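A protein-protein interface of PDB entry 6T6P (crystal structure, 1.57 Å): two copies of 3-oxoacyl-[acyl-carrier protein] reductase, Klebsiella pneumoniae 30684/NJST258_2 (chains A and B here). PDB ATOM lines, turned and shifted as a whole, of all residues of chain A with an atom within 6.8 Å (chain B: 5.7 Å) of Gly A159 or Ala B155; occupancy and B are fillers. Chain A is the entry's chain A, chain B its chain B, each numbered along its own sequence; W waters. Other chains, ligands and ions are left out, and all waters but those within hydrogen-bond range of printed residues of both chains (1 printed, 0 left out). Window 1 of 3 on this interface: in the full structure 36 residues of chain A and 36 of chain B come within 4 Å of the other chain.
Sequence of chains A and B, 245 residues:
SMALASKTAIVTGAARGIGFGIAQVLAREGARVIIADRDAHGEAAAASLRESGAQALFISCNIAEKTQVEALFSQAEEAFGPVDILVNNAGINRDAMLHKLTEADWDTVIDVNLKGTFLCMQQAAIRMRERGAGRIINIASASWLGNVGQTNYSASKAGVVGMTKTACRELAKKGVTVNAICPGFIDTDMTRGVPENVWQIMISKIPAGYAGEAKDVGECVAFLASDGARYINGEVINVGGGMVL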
ATOM      1  N   LEU A 114     -10.115 -25.761  -1.857  1.00  0.00           N
ATOM      2  CA  LEU A 114      -9.149 -24.746  -1.481  1.00  0.00           C
ATOM      3  C   LEU A 114      -8.060 -24.606  -2.545  1.00  0.00           C
ATOM      4  O   LEU A 114      -7.888 -23.507  -3.115  1.00  0.00           O
ATOM      5  CB  LEU A 114      -8.598 -25.034  -0.068  1.00  0.00           C
ATOM      6  CG  LEU A 114      -7.658 -23.966   0.494  1.00  0.00           C
ATOM      7  CD1 LEU A 114      -8.320 -22.576   0.546  1.00  0.00           C
ATOM      8  CD2 LEU A 114      -7.077 -24.376   1.843  1.00  0.00           C
ATOM      9  N   TRP A 144     -18.073 -21.332   6.881  1.00  0.00           N
ATOM     10  CA  TRP A 144     -16.691 -20.905   7.075  1.00  0.00           C
ATOM     11  C   TRP A 144     -16.396 -20.553   8.532  1.00  0.00           C
ATOM     12  O   TRP A 144     -15.217 -20.604   8.933  1.00  0.00           O
ATOM     13  CB  TRP A 144     -16.291 -19.742   6.159  1.00  0.00           C
ATOM     14  CG  TRP A 144     -16.713 -18.350   6.554  1.00  0.00           C
ATOM     15  CD1 TRP A 144     -17.962 -17.790   6.478  1.00  0.00           C
ATOM     16  CD2 TRP A 144     -15.835 -17.291   6.990  1.00  0.00           C
ATOM     17  NE1 TRP A 144     -17.924 -16.455   6.844  1.00  0.00           N
ATOM     18  CE2 TRP A 144     -16.621 -16.138   7.160  1.00  0.00           C
ATOM     19  CE3 TRP A 144     -14.467 -17.225   7.270  1.00  0.00           C
ATOM     20  CZ2 TRP A 144     -16.066 -14.906   7.587  1.00  0.00           C
ATOM     21  CZ3 TRP A 144     -13.922 -16.003   7.636  1.00  0.00           C
ATOM     22  CH2 TRP A 144     -14.704 -14.899   7.800  1.00  0.00           C
ATOM     23  N   TYR A 153     -14.639 -29.144   5.178  1.00  0.00           N
ATOM     24  CA  TYR A 153     -15.364 -28.148   4.358  1.00  0.00           C
ATOM     25  C   TYR A 153     -15.202 -26.751   4.937  1.00  0.00           C
ATOM     26  O   TYR A 153     -14.883 -25.799   4.192  1.00  0.00           O
ATOM     27  CB  TYR A 153     -16.846 -28.541   4.280  1.00  0.00           C
ATOM     28  CG  TYR A 153     -17.618 -27.739   3.271  1.00  0.00           C
ATOM     29  CD1 TYR A 153     -17.523 -28.039   1.926  1.00  0.00           C
ATOM     30  CD2 TYR A 153     -18.481 -26.743   3.679  1.00  0.00           C
ATOM     31  CE1 TYR A 153     -18.262 -27.327   0.986  1.00  0.00           C
ATOM     32  CE2 TYR A 153     -19.218 -26.041   2.760  1.00  0.00           C
ATOM     33  CZ  TYR A 153     -19.105 -26.345   1.436  1.00  0.00           C
ATOM     34  OH  TYR A 153     -19.856 -25.605   0.499  1.00  0.00           O
ATOM     35  N   SER A 154     -15.367 -26.616   6.234  1.00  0.00           N
ATOM     36  CA  SER A 154     -15.180 -25.310   6.896  1.00  0.00           C
ATOM     37  C   SER A 154     -13.737 -24.810   6.770  1.00  0.00           C
ATOM     38  O   SER A 154     -13.496 -23.630   6.514  1.00  0.00           O
ATOM     39  CB  SER A 154     -15.624 -25.348   8.377  1.00  0.00           C
ATOM     40  OG  SER A 154     -14.772 -26.180   9.174  1.00  0.00           O
ATOM     41  N   ALA A 155     -12.769 -25.708   6.881  1.00  0.00           N
ATOM     42  CA  ALA A 155     -11.369 -25.330   6.650  1.00  0.00           C
ATOM     43  C   ALA A 155     -11.220 -24.767   5.263  1.00  0.00           C
ATOM     44  O   ALA A 155     -10.565 -23.720   5.063  1.00  0.00           O
ATOM     45  CB  ALA A 155     -10.425 -26.495   6.835  1.00  0.00           C
ATOM     46  N   SER A 156     -11.768 -25.489   4.289  1.00  0.00           N
ATOM     47  CA  SER A 156     -11.583 -25.094   2.903  1.00  0.00           C
ATOM     48  C   SER A 156     -12.242 -23.722   2.617  1.00  0.00           C
ATOM     49  O   SER A 156     -11.670 -22.865   1.923  1.00  0.00           O
ATOM     50  CB  SER A 156     -12.080 -26.169   1.952  1.00  0.00           C
ATOM     51  OG  SER A 156     -13.506 -26.210   1.845  1.00  0.00           O
ATOM     52  N   LYS A 157     -13.435 -23.503   3.135  1.00  0.00           N
ATOM     53  CA  LYS A 157     -14.151 -22.276   2.806  1.00  0.00           C
ATOM     54  C   LYS A 157     -13.657 -21.065   3.596  1.00  0.00           C
ATOM     55  O   LYS A 157     -13.609 -19.947   3.077  1.00  0.00           O
ATOM     56  CB  LYS A 157     -15.667 -22.500   3.035  1.00  0.00           C
ATOM     57  CG  LYS A 157     -16.272 -23.522   2.063  1.00  0.00           C
ATOM     58  CD  LYS A 157     -16.196 -23.022   0.617  1.00  0.00           C
ATOM     59  CE  LYS A 157     -17.201 -23.698  -0.334  1.00  0.00           C
ATOM     60  NZ  LYS A 157     -17.099 -23.091  -1.663  1.00  0.00           N
ATOM     61  N   ALA A 158     -13.244 -21.277   4.851  1.00  0.00           N
ATOM     62  CA  ALA A 158     -12.522 -20.195   5.567  1.00  0.00           C
ATOM     63  C   ALA A 158     -11.224 -19.881   4.852  1.00  0.00           C
ATOM     64  O   ALA A 158     -10.861 -18.712   4.700  1.00  0.00           O
ATOM     65  CB  ALA A 158     -12.244 -20.571   7.025  1.00  0.00           C
ATOM     66  N   GLY A 159     -10.520 -20.887   4.360  1.00  0.00           N
ATOM     67  CA  GLY A 159      -9.313 -20.638   3.598  1.00  0.00           C
ATOM     68  C   GLY A 159      -9.554 -19.801   2.367  1.00  0.00           C
ATOM     69  O   GLY A 159      -8.735 -18.902   2.053  1.00  0.00           O
ATOM     70  N   VAL A 160     -10.668 -20.031   1.703  1.00  0.00           N
ATOM     71  CA  VAL A 160     -11.070 -19.195   0.537  1.00  0.00           C
ATOM     72  C   VAL A 160     -11.247 -17.735   0.953  1.00  0.00           C
ATOM     73  O   VAL A 160     -10.832 -16.830   0.258  1.00  0.00           O
ATOM     74  CB  VAL A 160     -12.307 -19.779  -0.163  1.00  0.00           C
ATOM     75  CG1 VAL A 160     -12.947 -18.774  -1.127  1.00  0.00           C
ATOM     76  CG2 VAL A 160     -11.915 -21.067  -0.873  1.00  0.00           C
ATOM     77  N   VAL A 161     -11.849 -17.490   2.105  1.00  0.00           N
ATOM     78  CA  VAL A 161     -11.969 -16.106   2.598  1.00  0.00           C
ATOM     79  C   VAL A 161     -10.608 -15.468   2.836  1.00  0.00           C
ATOM     80  O   VAL A 161     -10.371 -14.326   2.402  1.00  0.00           O
ATOM     81  CB  VAL A 161     -12.880 -16.031   3.865  1.00  0.00           C
ATOM     82  CG1 VAL A 161     -12.815 -14.646   4.444  1.00  0.00           C
ATOM     83  CG2 VAL A 161     -14.301 -16.424   3.515  1.00  0.00           C
ATOM     84  N   GLY A 162      -9.677 -16.201   3.453  1.00  0.00           N
ATOM     85  CA  GLY A 162      -8.339 -15.636   3.649  1.00  0.00           C
ATOM     86  C   GLY A 162      -7.701 -15.301   2.315  1.00  0.00           C
ATOM     87  O   GLY A 162      -7.057 -14.213   2.155  1.00  0.00           O
ATOM     88  N   MET A 163      -7.835 -16.163   1.313  1.00  0.00           N
ATOM     89  CA  MET A 163      -7.197 -15.892   0.038  1.00  0.00           C
ATOM     90  C   MET A 163      -7.867 -14.690  -0.651  1.00  0.00           C
ATOM     91  O   MET A 163      -7.201 -13.931  -1.379  1.00  0.00           O
ATOM     92  CB  MET A 163      -7.303 -17.089  -0.937  1.00  0.00           C
ATOM     93  CG  MET A 163      -6.550 -18.313  -0.431  1.00  0.00           C
ATOM     94  SD  MET A 163      -6.308 -19.562  -1.717  1.00  0.00           S
ATOM     95  CE  MET A 163      -8.012 -19.989  -2.099  1.00  0.00           C
ATOM     96  N   THR A 164      -9.180 -14.565  -0.491  1.00  0.00           N
ATOM     97  CA  THR A 164      -9.926 -13.445  -1.071  1.00  0.00           C
ATOM     98  C   THR A 164      -9.338 -12.131  -0.595  1.00  0.00           C
ATOM     99  O   THR A 164      -9.095 -11.198  -1.362  1.00  0.00           O
ATOM    100  CB  THR A 164     -11.421 -13.547  -0.662  1.00  0.00           C
ATOM    101  OG1 THR A 164     -11.992 -14.786  -1.141  1.00  0.00           O
ATOM    102  CG2 THR A 164     -12.214 -12.384  -1.186  1.00  0.00           C
ATOM    103  N   THR A 166      -6.350 -11.572   0.872  1.00  0.00           N
ATOM    104  CA  THR A 166      -4.984 -11.407   0.367  1.00  0.00           C
ATOM    105  C   THR A 166      -4.959 -10.890  -1.087  1.00  0.00           C
ATOM    106  O   THR A 166      -4.182  -9.986  -1.417  1.00  0.00           O
ATOM    107  CB  THR A 166      -4.235 -12.743   0.489  1.00  0.00           C
ATOM    108  OG1 THR A 166      -4.034 -12.978   1.882  1.00  0.00           O
ATOM    109  CG2 THR A 166      -2.891 -12.670  -0.192  1.00  0.00           C
ATOM    110  N   TRP B 106       2.725 -23.717  -2.319  1.00  0.00           N
ATOM    111  CA  TRP B 106       1.349 -23.879  -1.879  1.00  0.00           C
ATOM    112  C   TRP B 106       1.231 -25.154  -1.047  1.00  0.00           C
ATOM    113  O   TRP B 106       0.757 -25.132   0.112  1.00  0.00           O
ATOM    114  CB  TRP B 106       0.377 -23.899  -3.097  1.00  0.00           C
ATOM    115  CG  TRP B 106      -0.976 -24.348  -2.641  1.00  0.00           C
ATOM    116  CD1 TRP B 106      -1.410 -25.643  -2.597  1.00  0.00           C
ATOM    117  CD2 TRP B 106      -2.036 -23.554  -2.090  1.00  0.00           C
ATOM    118  NE1 TRP B 106      -2.640 -25.713  -2.032  1.00  0.00           N
ATOM    119  CE2 TRP B 106      -3.090 -24.445  -1.773  1.00  0.00           C
ATOM    120  CE3 TRP B 106      -2.256 -22.169  -1.935  1.00  0.00           C
ATOM    121  CZ2 TRP B 106      -4.261 -24.025  -1.205  1.00  0.00           C
ATOM    122  CZ3 TRP B 106      -3.430 -21.743  -1.380  1.00  0.00           C
ATOM    123  CH2 TRP B 106      -4.419 -22.676  -0.993  1.00  0.00           C
ATOM    124  N   ILE B 110       0.206 -25.593   3.134  1.00  0.00           N
ATOM    125  CA  ILE B 110      -1.079 -26.189   3.504  1.00  0.00           C
ATOM    126  C   ILE B 110      -0.824 -27.487   4.280  1.00  0.00           C
ATOM    127  O   ILE B 110      -1.510 -27.735   5.284  1.00  0.00           O
ATOM    128  CB  ILE B 110      -1.946 -26.440   2.274  1.00  0.00           C
ATOM    129  CG1 ILE B 110      -2.358 -25.162   1.605  1.00  0.00           C
ATOM    130  CG2 ILE B 110      -3.167 -27.335   2.571  1.00  0.00           C
ATOM    131  CD1 ILE B 110      -2.996 -24.126   2.379  1.00  0.00           C
ATOM    132  N   LEU B 114      -2.094 -26.414   7.878  1.00  0.00           N
ATOM    133  CA  LEU B 114      -3.516 -26.727   7.905  1.00  0.00           C
ATOM    134  C   LEU B 114      -3.747 -28.219   8.148  1.00  0.00           C
ATOM    135  O   LEU B 114      -4.384 -28.595   9.140  1.00  0.00           O
ATOM    136  CB  LEU B 114      -4.212 -26.215   6.619  1.00  0.00           C
ATOM    137  CG  LEU B 114      -5.750 -26.430   6.587  1.00  0.00           C
ATOM    138  CD1 LEU B 114      -6.433 -25.677   7.704  1.00  0.00           C
ATOM    139  CD2 LEU B 114      -6.308 -26.065   5.198  1.00  0.00           C
ATOM    140  N   GLN B 150       0.902 -13.680   0.911  1.00  0.00           N
ATOM    141  CA  GLN B 150       0.592 -14.786   1.801  1.00  0.00           C
ATOM    142  C   GLN B 150      -0.700 -15.492   1.413  1.00  0.00           C
ATOM    143  O   GLN B 150      -1.439 -15.951   2.260  1.00  0.00           O
ATOM    144  CB  GLN B 150       0.566 -14.320   3.254  1.00  0.00           C
ATOM    145  CG  GLN B 150       1.959 -13.886   3.676  1.00  0.00           C
ATOM    146  CD  GLN B 150       2.088 -13.705   5.194  1.00  0.00           C
ATOM    147  OE1 GLN B 150       1.142 -13.409   5.905  1.00  0.00           O
ATOM    148  NE2 GLN B 150       3.305 -13.860   5.683  1.00  0.00           N
ATOM    149  N   THR B 151      -0.912 -15.678   0.101  1.00  0.00           N
ATOM    150  CA  THR B 151      -2.038 -16.495  -0.346  1.00  0.00           C
ATOM    151  C   THR B 151      -2.100 -17.847   0.390  1.00  0.00           C
ATOM    152  O   THR B 151      -3.162 -18.233   0.928  1.00  0.00           O
ATOM    153  CB  THR B 151      -1.972 -16.715  -1.877  1.00  0.00           C
ATOM    154  OG1 THR B 151      -2.250 -15.494  -2.569  1.00  0.00           O
ATOM    155  CG2 THR B 151      -2.986 -17.739  -2.327  1.00  0.00           C
ATOM    156  N   ASN B 152      -0.981 -18.588   0.350  1.00  0.00           N
ATOM    157  CA  ASN B 152      -0.942 -19.916   1.027  1.00  0.00           C
ATOM    158  C   ASN B 152      -1.062 -19.830   2.534  1.00  0.00           C
ATOM    159  O   ASN B 152      -1.789 -20.563   3.161  1.00  0.00           O
ATOM    160  CB  ASN B 152       0.283 -20.738   0.581  1.00  0.00           C
ATOM    161  CG  ASN B 152       1.624 -20.014   0.694  1.00  0.00           C
ATOM    162  OD1 ASN B 152       1.710 -18.852   1.086  1.00  0.00           O
ATOM    163  ND2 ASN B 152       2.692 -20.710   0.387  1.00  0.00           N
ATOM    164  N   TYR B 153      -0.305 -18.888   3.125  1.00  0.00           N
ATOM    165  CA  TYR B 153      -0.272 -18.761   4.587  1.00  0.00           C
ATOM    166  C   TYR B 153      -1.599 -18.312   5.139  1.00  0.00           C
ATOM    167  O   TYR B 153      -2.133 -18.891   6.080  1.00  0.00           O
ATOM    168  CB  TYR B 153       0.868 -17.817   4.991  1.00  0.00           C
ATOM    169  CG  TYR B 153       1.155 -17.814   6.458  1.00  0.00           C
ATOM    170  CD1 TYR B 153       1.895 -18.836   7.035  1.00  0.00           C
ATOM    171  CD2 TYR B 153       0.757 -16.757   7.241  1.00  0.00           C
ATOM    172  CE1 TYR B 153       2.206 -18.798   8.406  1.00  0.00           C
ATOM    173  CE2 TYR B 153       1.044 -16.756   8.597  1.00  0.00           C
ATOM    174  CZ  TYR B 153       1.751 -17.758   9.138  1.00  0.00           C
ATOM    175  OH  TYR B 153       2.106 -17.724  10.517  1.00  0.00           O
ATOM    176  N   SER B 154      -2.174 -17.280   4.495  1.00  0.00           N
ATOM    177  CA  SER B 154      -3.509 -16.828   4.914  1.00  0.00           C
ATOM    178  C   SER B 154      -4.573 -17.882   4.731  1.00  0.00           C
ATOM    179  O   SER B 154      -5.437 -18.063   5.587  1.00  0.00           O
ATOM    180  CB  SER B 154      -3.905 -15.516   4.180  1.00  0.00           C
ATOM    181  OG  SER B 154      -4.117 -15.702   2.788  1.00  0.00           O
ATOM    182  N   ALA B 155      -4.514 -18.624   3.626  1.00  0.00           N
ATOM    183  CA  ALA B 155      -5.445 -19.756   3.456  1.00  0.00           C
ATOM    184  C   ALA B 155      -5.324 -20.717   4.611  1.00  0.00           C
ATOM    185  O   ALA B 155      -6.330 -21.181   5.158  1.00  0.00           O
ATOM    186  CB  ALA B 155      -5.203 -20.484   2.157  1.00  0.00           C
ATOM    187  N   SER B 156      -4.091 -21.079   4.935  1.00  0.00           N
ATOM    188  CA  SER B 156      -3.851 -22.071   5.957  1.00  0.00           C
ATOM    189  C   SER B 156      -4.365 -21.606   7.330  1.00  0.00           C
ATOM    190  O   SER B 156      -5.007 -22.377   8.070  1.00  0.00           O
ATOM    191  CB  SER B 156      -2.388 -22.489   6.030  1.00  0.00           C
ATOM    192  OG  SER B 156      -1.561 -21.529   6.646  1.00  0.00           O
ATOM    193  N   LYS B 157      -4.111 -20.354   7.674  1.00  0.00           N
ATOM    194  CA  LYS B 157      -4.451 -19.887   9.025  1.00  0.00           C
ATOM    195  C   LYS B 157      -5.920 -19.540   9.155  1.00  0.00           C
ATOM    196  O   LYS B 157      -6.529 -19.771  10.211  1.00  0.00           O
ATOM    197  CB  LYS B 157      -3.533 -18.697   9.345  1.00  0.00           C
ATOM    198  CG  LYS B 157      -2.081 -19.012   9.497  1.00  0.00           C
ATOM    199  CD  LYS B 157      -1.822 -19.995  10.651  1.00  0.00           C
ATOM    200  CE  LYS B 157      -0.366 -19.973  11.179  1.00  0.00           C
ATOM    201  NZ  LYS B 157      -0.242 -20.869  12.364  1.00  0.00           N
ATOM    202  N   ALA B 158      -6.557 -19.025   8.091  1.00  0.00           N
ATOM    203  CA  ALA B 158      -8.007 -18.907   8.090  1.00  0.00           C
ATOM    204  C   ALA B 158      -8.640 -20.277   8.172  1.00  0.00           C
ATOM    205  O   ALA B 158      -9.632 -20.468   8.903  1.00  0.00           O
ATOM    206  CB  ALA B 158      -8.525 -18.176   6.830  1.00  0.00           C
ATOM    207  N   GLY B 159      -8.098 -21.264   7.483  1.00  0.00           N
ATOM    208  CA  GLY B 159      -8.624 -22.599   7.567  1.00  0.00           C
ATOM    209  C   GLY B 159      -8.572 -23.147   8.989  1.00  0.00           C
ATOM    210  O   GLY B 159      -9.553 -23.818   9.422  1.00  0.00           O
ATOM    211  N   VAL B 160      -7.504 -22.841   9.709  1.00  0.00           N
ATOM    212  CA  VAL B 160      -7.400 -23.227  11.133  1.00  0.00           C
ATOM    213  C   VAL B 160      -8.527 -22.609  11.941  1.00  0.00           C
ATOM    214  O   VAL B 160      -9.104 -23.233  12.823  1.00  0.00           O
ATOM    215  CB  VAL B 160      -5.989 -22.862  11.694  1.00  0.00           C
ATOM    216  CG1 VAL B 160      -5.959 -22.944  13.227  1.00  0.00           C
ATOM    217  CG2 VAL B 160      -4.980 -23.833  11.113  1.00  0.00           C
HETATM  218  O   HOH W   1      -4.938 -14.901  -3.013  1.00  0.00           O
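Among the printed residues, pairs that only touch across the chains: Ala A158 with Ala B158 (3.2 Å), Ala A155 with Gly B159 (3.4 Å), Gly A159 with Ala B155 (3.4 Å), Thr A166 with Thr B151 (3.6 Å), Met A163 with Trp B106 (3.6 Å), Met A163 with Ala B155 (3.6 Å), Met A163 with Thr B151 (3.7 Å), Leu A114 with Trp B106 (3.8 Å), Leu A114 with Leu B114 (3.8 Å), Thr A166 with Gln B150 (3.9 Å) and Gly A159 with Gly B159 (3.97 Å).
Of the printed residues of chain B, Leu A114 touches Trp B106 and Leu B114.
Gly A159 touches two residues of chain B.
Printed residues of chain B within 4 Å of Thr A166: Gln B150, Thr B151 and Ser B154.
Of the printed residues of chain A, Gln B150 touches Thr A166.
Printed residues of chain A within 4 Å of Thr B151: Met A163 and Thr A166.
Ala B155 touches two residues of chain A.
Printed residues of chain A within 4 Å of Gly B159: Ala A155 (3.4 Å) and Gly A159 (3.97 Å).
The nearest residue of chain B that does not touch Gly A159 is Ala B158 (4.1 Å).
The backbone carbonyl oxygen (O) of Gly A162 is in hydrogen-bond range of the side-chain hydroxyl (OG) of Ser B154 (3.4 Å).
The side-chain hydroxyl (OG1) of Thr A166 is in hydrogen-bond range of the side-chain hydroxyl (OG) of Ser B154 (2.9 Å).
Water W1 lies within hydrogen-bond range of OG1 of Thr B151 and O of Met A163.
The backbone carbonyl oxygen of Gly A162 sits at hydrogen-bond distance from the side-chain hydroxyl of Thr A166, 3.3 Å away.
The backbone carbonyl oxygen (O) of Gln B150 lies within hydrogen-bond range of the side-chain hydroxyl (OG) of Ser B154 (2.7 Å).
The backbone carbonyl oxygen (O) of Thr B151 is in hydrogen-bond range of the side-chain hydroxyl (OG) of Ser B154.
Leu B114 touches its own counterpart, Leu A114.
Ala A155 touches Gly B159, and with the chains exchanged Gly A159 touches Ala B155.
Ala B158 touches its own counterpart, Ala A158.
Gly B159 touches its own counterpart, Gly A159.
Positions printed for both chains: 114, 153, 154, 155, 156, 157, 158, 159 and 160.
Of the 13 pairs that touch across the chains among the printed residues, 5 have their exchanged pair printed and touching as well.
Hydrophobic or aromatic side chains of chain A that line the printed part of chain B: Leu A114, Ala A155, Ala A158 and Met A163.
Of the 14 printed residues of chain B, 8 touch a printed residue of chain A.
Among the printed residues, 13 pairs touch across the chains.
Among the printed residues, no Asp or Glu carboxylate lies within 4 Å of a Lys or Arg side-chain nitrogen of the other chain.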
